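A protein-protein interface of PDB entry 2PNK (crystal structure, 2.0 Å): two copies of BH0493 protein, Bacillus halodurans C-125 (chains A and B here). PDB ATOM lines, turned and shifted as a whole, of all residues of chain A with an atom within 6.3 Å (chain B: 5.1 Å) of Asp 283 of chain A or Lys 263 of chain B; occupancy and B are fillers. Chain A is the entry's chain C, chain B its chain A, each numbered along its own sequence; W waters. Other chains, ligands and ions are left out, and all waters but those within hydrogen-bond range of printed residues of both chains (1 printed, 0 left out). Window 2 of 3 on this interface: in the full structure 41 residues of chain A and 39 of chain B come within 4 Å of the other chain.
Among the printed residues, pairs that only touch across the chains: Glu 286 of chain A with Val 266 of chain B, Glu 286 of chain A with Phe 276 of chain B and Met 282 of chain A with Phe 276 of chain B.
Of the 11 printed residues of chain B, 3 touch a printed residue of chain A. Printed residues of chain B that touch a printed residue of chain A: Lys 263, Val 266 and Phe 276. Of the 11 printed residues of chain A, 4 touch a printed residue of chain B. Hydrophobic or aromatic side chains of chain A that line the printed part of chain B: Met 282. Among the printed residues, 6 pairs touch across the chains. Among the printed residues, Asp or Glu carboxylates within 4 Å of a Lys or Arg side-chain nitrogen of the other chain: Asp 283 of chain A with Lys 263 of chain B and Glu 286 of chain A with Lys 263 of chain B.
No position is printed for both chains. Of the 6 pairs that touch across the chains among the printed residues, none has its exchanged pair printed and touching as well.
O of Lys 263 of chain B is in hydrogen-bond range of N of Phe 276 of chain B (2.9 Å). The backbone NH (N) of Val 266 of chain B sits at hydrogen-bond distance from the backbone carbonyl oxygen (O) of Gly 274 of chain B (2.9 Å). The side-chain hydroxyl (OG) of Ser 281 of chain A is in hydrogen-bond range of the backbone NH (N) of Asp 283 of chain A (3.1 Å). OE2 of Glu 286 of chain A is in salt-bridge range of NH1 of Arg 290 of chain A (3.0 Å).
Water W1 lies within hydrogen-bond range of OE1 of Glu 286 of chain A (2.6 Å), OD1 of Asp 283 of chain A (2.7 Å) and NZ of Lys 263 of chain B (3.3 Å).
Printed residues of chain B within 4 Å of Asp 283 of chain A: Lys 263 (3.5 Å). Of chain A, only Asp 283 and Glu 286 come within 4 Å of Lys 263 of chain B. Of the printed residues of chain B, Met 282 of chain A touches Phe 276 (3.997 Å). Of the printed residues of chain B, Arg 290 of chain A touches Val 266 (2.9 Å). Of the printed residues of chain A, Val 266 of chain B touches Glu 286 and Arg 290. The nearest residue of chain A that does not touch Lys 263 of chain B is Arg 290 of chain A (6.0 Å). The nearest printed residue of chain B that does not touch Met 282 of chain A is Val 277 of chain B (5.7 Å).
The side-chain carboxylate (OD1) of Asp 283 of chain A is in salt-bridge range of the side-chain amino group (NZ) of Lys 263 of chain B. OE1 of Glu 286 of chain A lies within salt-bridge range of NZ of Lys 263 of chain B, 2.7 Å away. The guanidinium group of Arg 290 of chain A lies within hydrogen-bond range of the backbone carbonyl oxygen of Val 266 of chain B (2.9 Å).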
ATOM      1  N   PHE A 231     -13.734  11.654   9.697  1.00  0.00           N
ATOM      2  CA  PHE A 231     -13.993  11.791   8.262  1.00  0.00           C
ATOM      3  C   PHE A 231     -13.781  13.250   7.860  1.00  0.00           C
ATOM      4  O   PHE A 231     -14.310  14.135   8.492  1.00  0.00           O
ATOM      5  CB  PHE A 231     -15.430  11.386   7.931  1.00  0.00           C
ATOM      6  CG  PHE A 231     -15.727  11.395   6.454  1.00  0.00           C
ATOM      7  CD1 PHE A 231     -16.068  12.572   5.802  1.00  0.00           C
ATOM      8  CD2 PHE A 231     -15.612  10.234   5.710  1.00  0.00           C
ATOM      9  CE1 PHE A 231     -16.307  12.578   4.428  1.00  0.00           C
ATOM     10  CE2 PHE A 231     -15.852  10.243   4.342  1.00  0.00           C
ATOM     11  CZ  PHE A 231     -16.199  11.419   3.708  1.00  0.00           C
ATOM     12  N   ALA A 280     -16.840  10.678  21.282  1.00  0.00           N
ATOM     13  CA  ALA A 280     -16.307  10.899  19.946  1.00  0.00           C
ATOM     14  C   ALA A 280     -16.164  12.382  19.617  1.00  0.00           C
ATOM     15  O   ALA A 280     -16.829  13.240  20.215  1.00  0.00           O
ATOM     16  CB  ALA A 280     -17.169  10.221  18.930  1.00  0.00           C
ATOM     17  N   SER A 281     -15.257  12.694  18.692  1.00  0.00           N
ATOM     18  CA  SER A 281     -15.188  14.055  18.127  1.00  0.00           C
ATOM     19  C   SER A 281     -16.421  14.221  17.278  1.00  0.00           C
ATOM     20  O   SER A 281     -16.871  13.264  16.702  1.00  0.00           O
ATOM     21  CB  SER A 281     -13.958  14.269  17.240  1.00  0.00           C
ATOM     22  OG  SER A 281     -14.029  15.534  16.608  1.00  0.00           O
ATOM     23  N   MET A 282     -16.996  15.417  17.253  1.00  0.00           N
ATOM     24  CA  MET A 282     -18.123  15.711  16.359  1.00  0.00           C
ATOM     25  C   MET A 282     -17.666  16.103  14.936  1.00  0.00           C
ATOM     26  O   MET A 282     -18.494  16.267  14.032  1.00  0.00           O
ATOM     27  CB  MET A 282     -18.953  16.857  16.941  1.00  0.00           C
ATOM     28  CG  MET A 282     -19.573  16.581  18.298  1.00  0.00           C
ATOM     29  SD  MET A 282     -20.690  14.984  18.346  1.00  0.00           S
ATOM     30  CE  MET A 282     -21.972  15.608  17.177  1.00  0.00           C
ATOM     31  N   ASP A 283     -16.362  16.266  14.741  1.00  0.00           N
ATOM     32  CA  ASP A 283     -15.824  16.858  13.508  1.00  0.00           C
ATOM     33  C   ASP A 283     -16.226  16.092  12.246  1.00  0.00           C
ATOM     34  O   ASP A 283     -16.579  16.704  11.226  1.00  0.00           O
ATOM     35  CB  ASP A 283     -14.289  16.891  13.546  1.00  0.00           C
ATOM     36  CG  ASP A 283     -13.736  17.983  14.446  1.00  0.00           C
ATOM     37  OD1 ASP A 283     -14.532  18.764  15.006  1.00  0.00           O
ATOM     38  OD2 ASP A 283     -12.488  18.045  14.598  1.00  0.00           O
ATOM     39  N   GLY A 284     -16.145  14.767  12.313  1.00  0.00           N
ATOM     40  CA  GLY A 284     -16.462  13.921  11.152  1.00  0.00           C
ATOM     41  C   GLY A 284     -17.925  13.998  10.766  1.00  0.00           C
ATOM     42  O   GLY A 284     -18.246  14.097   9.584  1.00  0.00           O
ATOM     43  N   VAL A 285     -18.798  13.978  11.781  1.00  0.00           N
ATOM     44  CA  VAL A 285     -20.242  14.110  11.585  1.00  0.00           C
ATOM     45  C   VAL A 285     -20.548  15.494  10.998  1.00  0.00           C
ATOM     46  O   VAL A 285     -21.286  15.617  10.040  1.00  0.00           O
ATOM     47  CB  VAL A 285     -21.028  13.922  12.929  1.00  0.00           C
ATOM     48  CG1 VAL A 285     -22.557  13.891  12.681  1.00  0.00           C
ATOM     49  CG2 VAL A 285     -20.573  12.616  13.684  1.00  0.00           C
ATOM     50  N   GLU A 286     -19.954  16.534  11.573  1.00  0.00           N
ATOM     51  CA  GLU A 286     -20.133  17.917  11.068  1.00  0.00           C
ATOM     52  C   GLU A 286     -19.719  18.019   9.599  1.00  0.00           C
ATOM     53  O   GLU A 286     -20.396  18.638   8.786  1.00  0.00           O
ATOM     54  CB  GLU A 286     -19.284  18.865  11.901  1.00  0.00           C
ATOM     55  CG  GLU A 286     -19.381  20.359  11.549  1.00  0.00           C
ATOM     56  CD  GLU A 286     -18.213  21.154  12.130  1.00  0.00           C
ATOM     57  OE1 GLU A 286     -17.733  20.812  13.234  1.00  0.00           O
ATOM     58  OE2 GLU A 286     -17.747  22.101  11.468  1.00  0.00           O
ATOM     59  N   HIS A 287     -18.576  17.431   9.274  1.00  0.00           N
ATOM     60  CA  HIS A 287     -18.056  17.463   7.915  1.00  0.00           C
ATOM     61  C   HIS A 287     -19.007  16.779   6.912  1.00  0.00           C
ATOM     62  O   HIS A 287     -19.334  17.342   5.851  1.00  0.00           O
ATOM     63  CB  HIS A 287     -16.673  16.812   7.859  1.00  0.00           C
ATOM     64  CG  HIS A 287     -16.035  16.921   6.509  1.00  0.00           C
ATOM     65  ND1 HIS A 287     -16.386  16.107   5.450  1.00  0.00           N
ATOM     66  CD2 HIS A 287     -15.115  17.790   6.025  1.00  0.00           C
ATOM     67  CE1 HIS A 287     -15.689  16.453   4.384  1.00  0.00           C
ATOM     68  NE2 HIS A 287     -14.906  17.467   4.707  1.00  0.00           N
ATOM     69  N   LEU A 288     -19.446  15.570   7.258  1.00  0.00           N
ATOM     70  CA  LEU A 288     -20.387  14.808   6.441  1.00  0.00           C
ATOM     71  C   LEU A 288     -21.660  15.615   6.181  1.00  0.00           C
ATOM     72  O   LEU A 288     -22.077  15.757   5.054  1.00  0.00           O
ATOM     73  CB  LEU A 288     -20.717  13.469   7.135  1.00  0.00           C
ATOM     74  CG  LEU A 288     -19.609  12.404   7.019  1.00  0.00           C
ATOM     75  CD1 LEU A 288     -19.777  11.264   8.040  1.00  0.00           C
ATOM     76  CD2 LEU A 288     -19.551  11.836   5.614  1.00  0.00           C
ATOM     77  N   ARG A 290     -22.247  18.934   6.374  1.00  0.00           N
ATOM     78  CA  ARG A 290     -22.009  20.147   5.580  1.00  0.00           C
ATOM     79  C   ARG A 290     -21.649  19.836   4.136  1.00  0.00           C
ATOM     80  O   ARG A 290     -22.161  20.466   3.229  1.00  0.00           O
ATOM     81  CB  ARG A 290     -20.876  20.977   6.183  1.00  0.00           C
ATOM     82  CG  ARG A 290     -20.553  22.239   5.395  1.00  0.00           C
ATOM     83  CD  ARG A 290     -19.604  23.181   6.103  1.00  0.00           C
ATOM     84  NE  ARG A 290     -18.381  22.501   6.534  1.00  0.00           N
ATOM     85  CZ  ARG A 290     -18.086  22.163   7.785  1.00  0.00           C
ATOM     86  NH1 ARG A 290     -18.913  22.443   8.775  1.00  0.00           N
ATOM     87  NH2 ARG A 290     -16.947  21.531   8.046  1.00  0.00           N
ATOM     88  N   PRO B 227     -13.445  26.687  21.167  1.00  0.00           N
ATOM     89  CA  PRO B 227     -13.108  25.602  22.063  1.00  0.00           C
ATOM     90  C   PRO B 227     -11.612  25.352  22.156  1.00  0.00           C
ATOM     91  O   PRO B 227     -11.164  24.813  23.145  1.00  0.00           O
ATOM     92  CB  PRO B 227     -13.811  24.401  21.440  1.00  0.00           C
ATOM     93  CG  PRO B 227     -14.802  24.942  20.516  1.00  0.00           C
ATOM     94  CD  PRO B 227     -14.330  26.252  20.069  1.00  0.00           C
ATOM     95  N   GLY B 261     -16.241  28.616  23.966  1.00  0.00           N
ATOM     96  CA  GLY B 261     -16.738  27.363  23.413  1.00  0.00           C
ATOM     97  C   GLY B 261     -17.479  27.462  22.108  1.00  0.00           C
ATOM     98  O   GLY B 261     -17.978  26.465  21.624  1.00  0.00           O
ATOM     99  N   VAL B 262     -17.556  28.652  21.506  1.00  0.00           N
ATOM    100  CA  VAL B 262     -18.272  28.796  20.222  1.00  0.00           C
ATOM    101  C   VAL B 262     -17.366  28.465  19.054  1.00  0.00           C
ATOM    102  O   VAL B 262     -16.265  28.992  18.933  1.00  0.00           O
ATOM    103  CB  VAL B 262     -18.920  30.190  20.031  1.00  0.00           C
ATOM    104  CG1 VAL B 262     -17.850  31.350  20.102  1.00  0.00           C
ATOM    105  CG2 VAL B 262     -19.709  30.230  18.717  1.00  0.00           C
ATOM    106  N   LYS B 263     -17.844  27.582  18.194  1.00  0.00           N
ATOM    107  CA  LYS B 263     -17.189  27.274  16.933  1.00  0.00           C
ATOM    108  C   LYS B 263     -17.952  27.990  15.804  1.00  0.00           C
ATOM    109  O   LYS B 263     -19.058  27.610  15.456  1.00  0.00           O
ATOM    110  CB  LYS B 263     -17.148  25.750  16.750  1.00  0.00           C
ATOM    111  CG  LYS B 263     -16.259  25.312  15.623  1.00  0.00           C
ATOM    112  CD  LYS B 263     -16.166  23.785  15.454  1.00  0.00           C
ATOM    113  CE  LYS B 263     -15.678  23.438  14.002  1.00  0.00           C
ATOM    114  NZ  LYS B 263     -15.373  21.991  13.823  1.00  0.00           N
ATOM    115  N   LYS B 264     -17.360  29.042  15.249  1.00  0.00           N
ATOM    116  CA  LYS B 264     -18.069  29.943  14.347  1.00  0.00           C
ATOM    117  C   LYS B 264     -18.339  29.334  12.967  1.00  0.00           C
ATOM    118  O   LYS B 264     -17.486  28.668  12.377  1.00  0.00           O
ATOM    119  CB  LYS B 264     -17.294  31.262  14.152  1.00  0.00           C
ATOM    120  CG  LYS B 264     -17.120  32.148  15.388  1.00  0.00           C
ATOM    121  CD  LYS B 264     -18.434  32.620  15.975  1.00  0.00           C
ATOM    122  CE  LYS B 264     -19.078  33.730  15.129  1.00  0.00           C
ATOM    123  NZ  LYS B 264     -20.443  34.004  15.635  1.00  0.00           N
ATOM    124  N   ARG B 265     -19.551  29.569  12.480  1.00  0.00           N
ATOM    125  CA  ARG B 265     -19.919  29.317  11.079  1.00  0.00           C
ATOM    126  C   ARG B 265     -19.645  27.917  10.556  1.00  0.00           C
ATOM    127  O   ARG B 265     -19.030  27.762   9.504  1.00  0.00           O
ATOM    128  CB  ARG B 265     -19.277  30.385  10.170  1.00  0.00           C
ATOM    129  CG  ARG B 265     -19.910  31.786  10.382  1.00  0.00           C
ATOM    130  CD  ARG B 265     -21.480  31.723  10.397  1.00  0.00           C
ATOM    131  NE  ARG B 265     -22.134  33.034  10.460  1.00  0.00           N
ATOM    132  CZ  ARG B 265     -22.230  33.783  11.563  1.00  0.00           C
ATOM    133  NH1 ARG B 265     -21.716  33.375  12.723  1.00  0.00           N
ATOM    134  NH2 ARG B 265     -22.861  34.951  11.509  1.00  0.00           N
ATOM    135  N   VAL B 266     -20.137  26.898  11.266  1.00  0.00           N
ATOM    136  CA  VAL B 266     -20.088  25.532  10.739  1.00  0.00           C
ATOM    137  C   VAL B 266     -21.148  25.320   9.638  1.00  0.00           C
ATOM    138  O   VAL B 266     -21.006  24.434   8.810  1.00  0.00           O
ATOM    139  CB  VAL B 266     -20.164  24.433  11.861  1.00  0.00           C
ATOM    140  CG1 VAL B 266     -19.276  24.821  13.004  1.00  0.00           C
ATOM    141  CG2 VAL B 266     -21.584  24.163  12.325  1.00  0.00           C
ATOM    142  N   GLY B 274     -25.735  29.750  12.420  1.00  0.00           N
ATOM    143  CA  GLY B 274     -24.750  28.756  11.932  1.00  0.00           C
ATOM    144  C   GLY B 274     -23.576  28.362  12.833  1.00  0.00           C
ATOM    145  O   GLY B 274     -22.654  27.676  12.397  1.00  0.00           O
ATOM    146  N   ASP B 275     -23.616  28.764  14.099  1.00  0.00           N
ATOM    147  CA  ASP B 275     -22.520  28.528  15.021  1.00  0.00           C
ATOM    148  C   ASP B 275     -22.755  27.285  15.887  1.00  0.00           C
ATOM    149  O   ASP B 275     -23.872  27.010  16.304  1.00  0.00           O
ATOM    150  CB  ASP B 275     -22.348  29.723  15.944  1.00  0.00           C
ATOM    151  CG  ASP B 275     -21.900  30.989  15.226  1.00  0.00           C
ATOM    152  OD1 ASP B 275     -21.351  30.900  14.098  1.00  0.00           O
ATOM    153  OD2 ASP B 275     -22.096  32.082  15.824  1.00  0.00           O
ATOM    154  N   PHE B 276     -21.661  26.601  16.188  1.00  0.00           N
ATOM    155  CA  PHE B 276     -21.660  25.299  16.885  1.00  0.00           C
ATOM    156  C   PHE B 276     -20.907  25.425  18.218  1.00  0.00           C
ATOM    157  O   PHE B 276     -20.550  26.523  18.646  1.00  0.00           O
ATOM    158  CB  PHE B 276     -21.047  24.262  15.942  1.00  0.00           C
ATOM    159  CG  PHE B 276     -21.178  22.822  16.377  1.00  0.00           C
ATOM    160  CD1 PHE B 276     -22.337  22.335  16.960  1.00  0.00           C
ATOM    161  CD2 PHE B 276     -20.132  21.943  16.141  1.00  0.00           C
ATOM    162  CE1 PHE B 276     -22.419  21.006  17.352  1.00  0.00           C
ATOM    163  CE2 PHE B 276     -20.218  20.623  16.504  1.00  0.00           C
ATOM    164  CZ  PHE B 276     -21.370  20.154  17.100  1.00  0.00           C
ATOM    165  N   VAL B 277     -20.705  24.296  18.892  1.00  0.00           N
ATOM    166  CA  VAL B 277     -20.121  24.250  20.202  1.00  0.00           C
ATOM    167  C   VAL B 277     -19.078  23.138  20.321  1.00  0.00           C
ATOM    168  O   VAL B 277     -19.179  22.087  19.678  1.00  0.00           O
ATOM    169  CB  VAL B 277     -21.226  24.021  21.278  1.00  0.00           C
ATOM    170  CG1 VAL B 277     -21.967  22.687  21.070  1.00  0.00           C
ATOM    171  CG2 VAL B 277     -20.648  24.081  22.667  1.00  0.00           C
HETATM  172  O   HOH W   1     -17.112  19.593  15.386  1.00  0.00           O
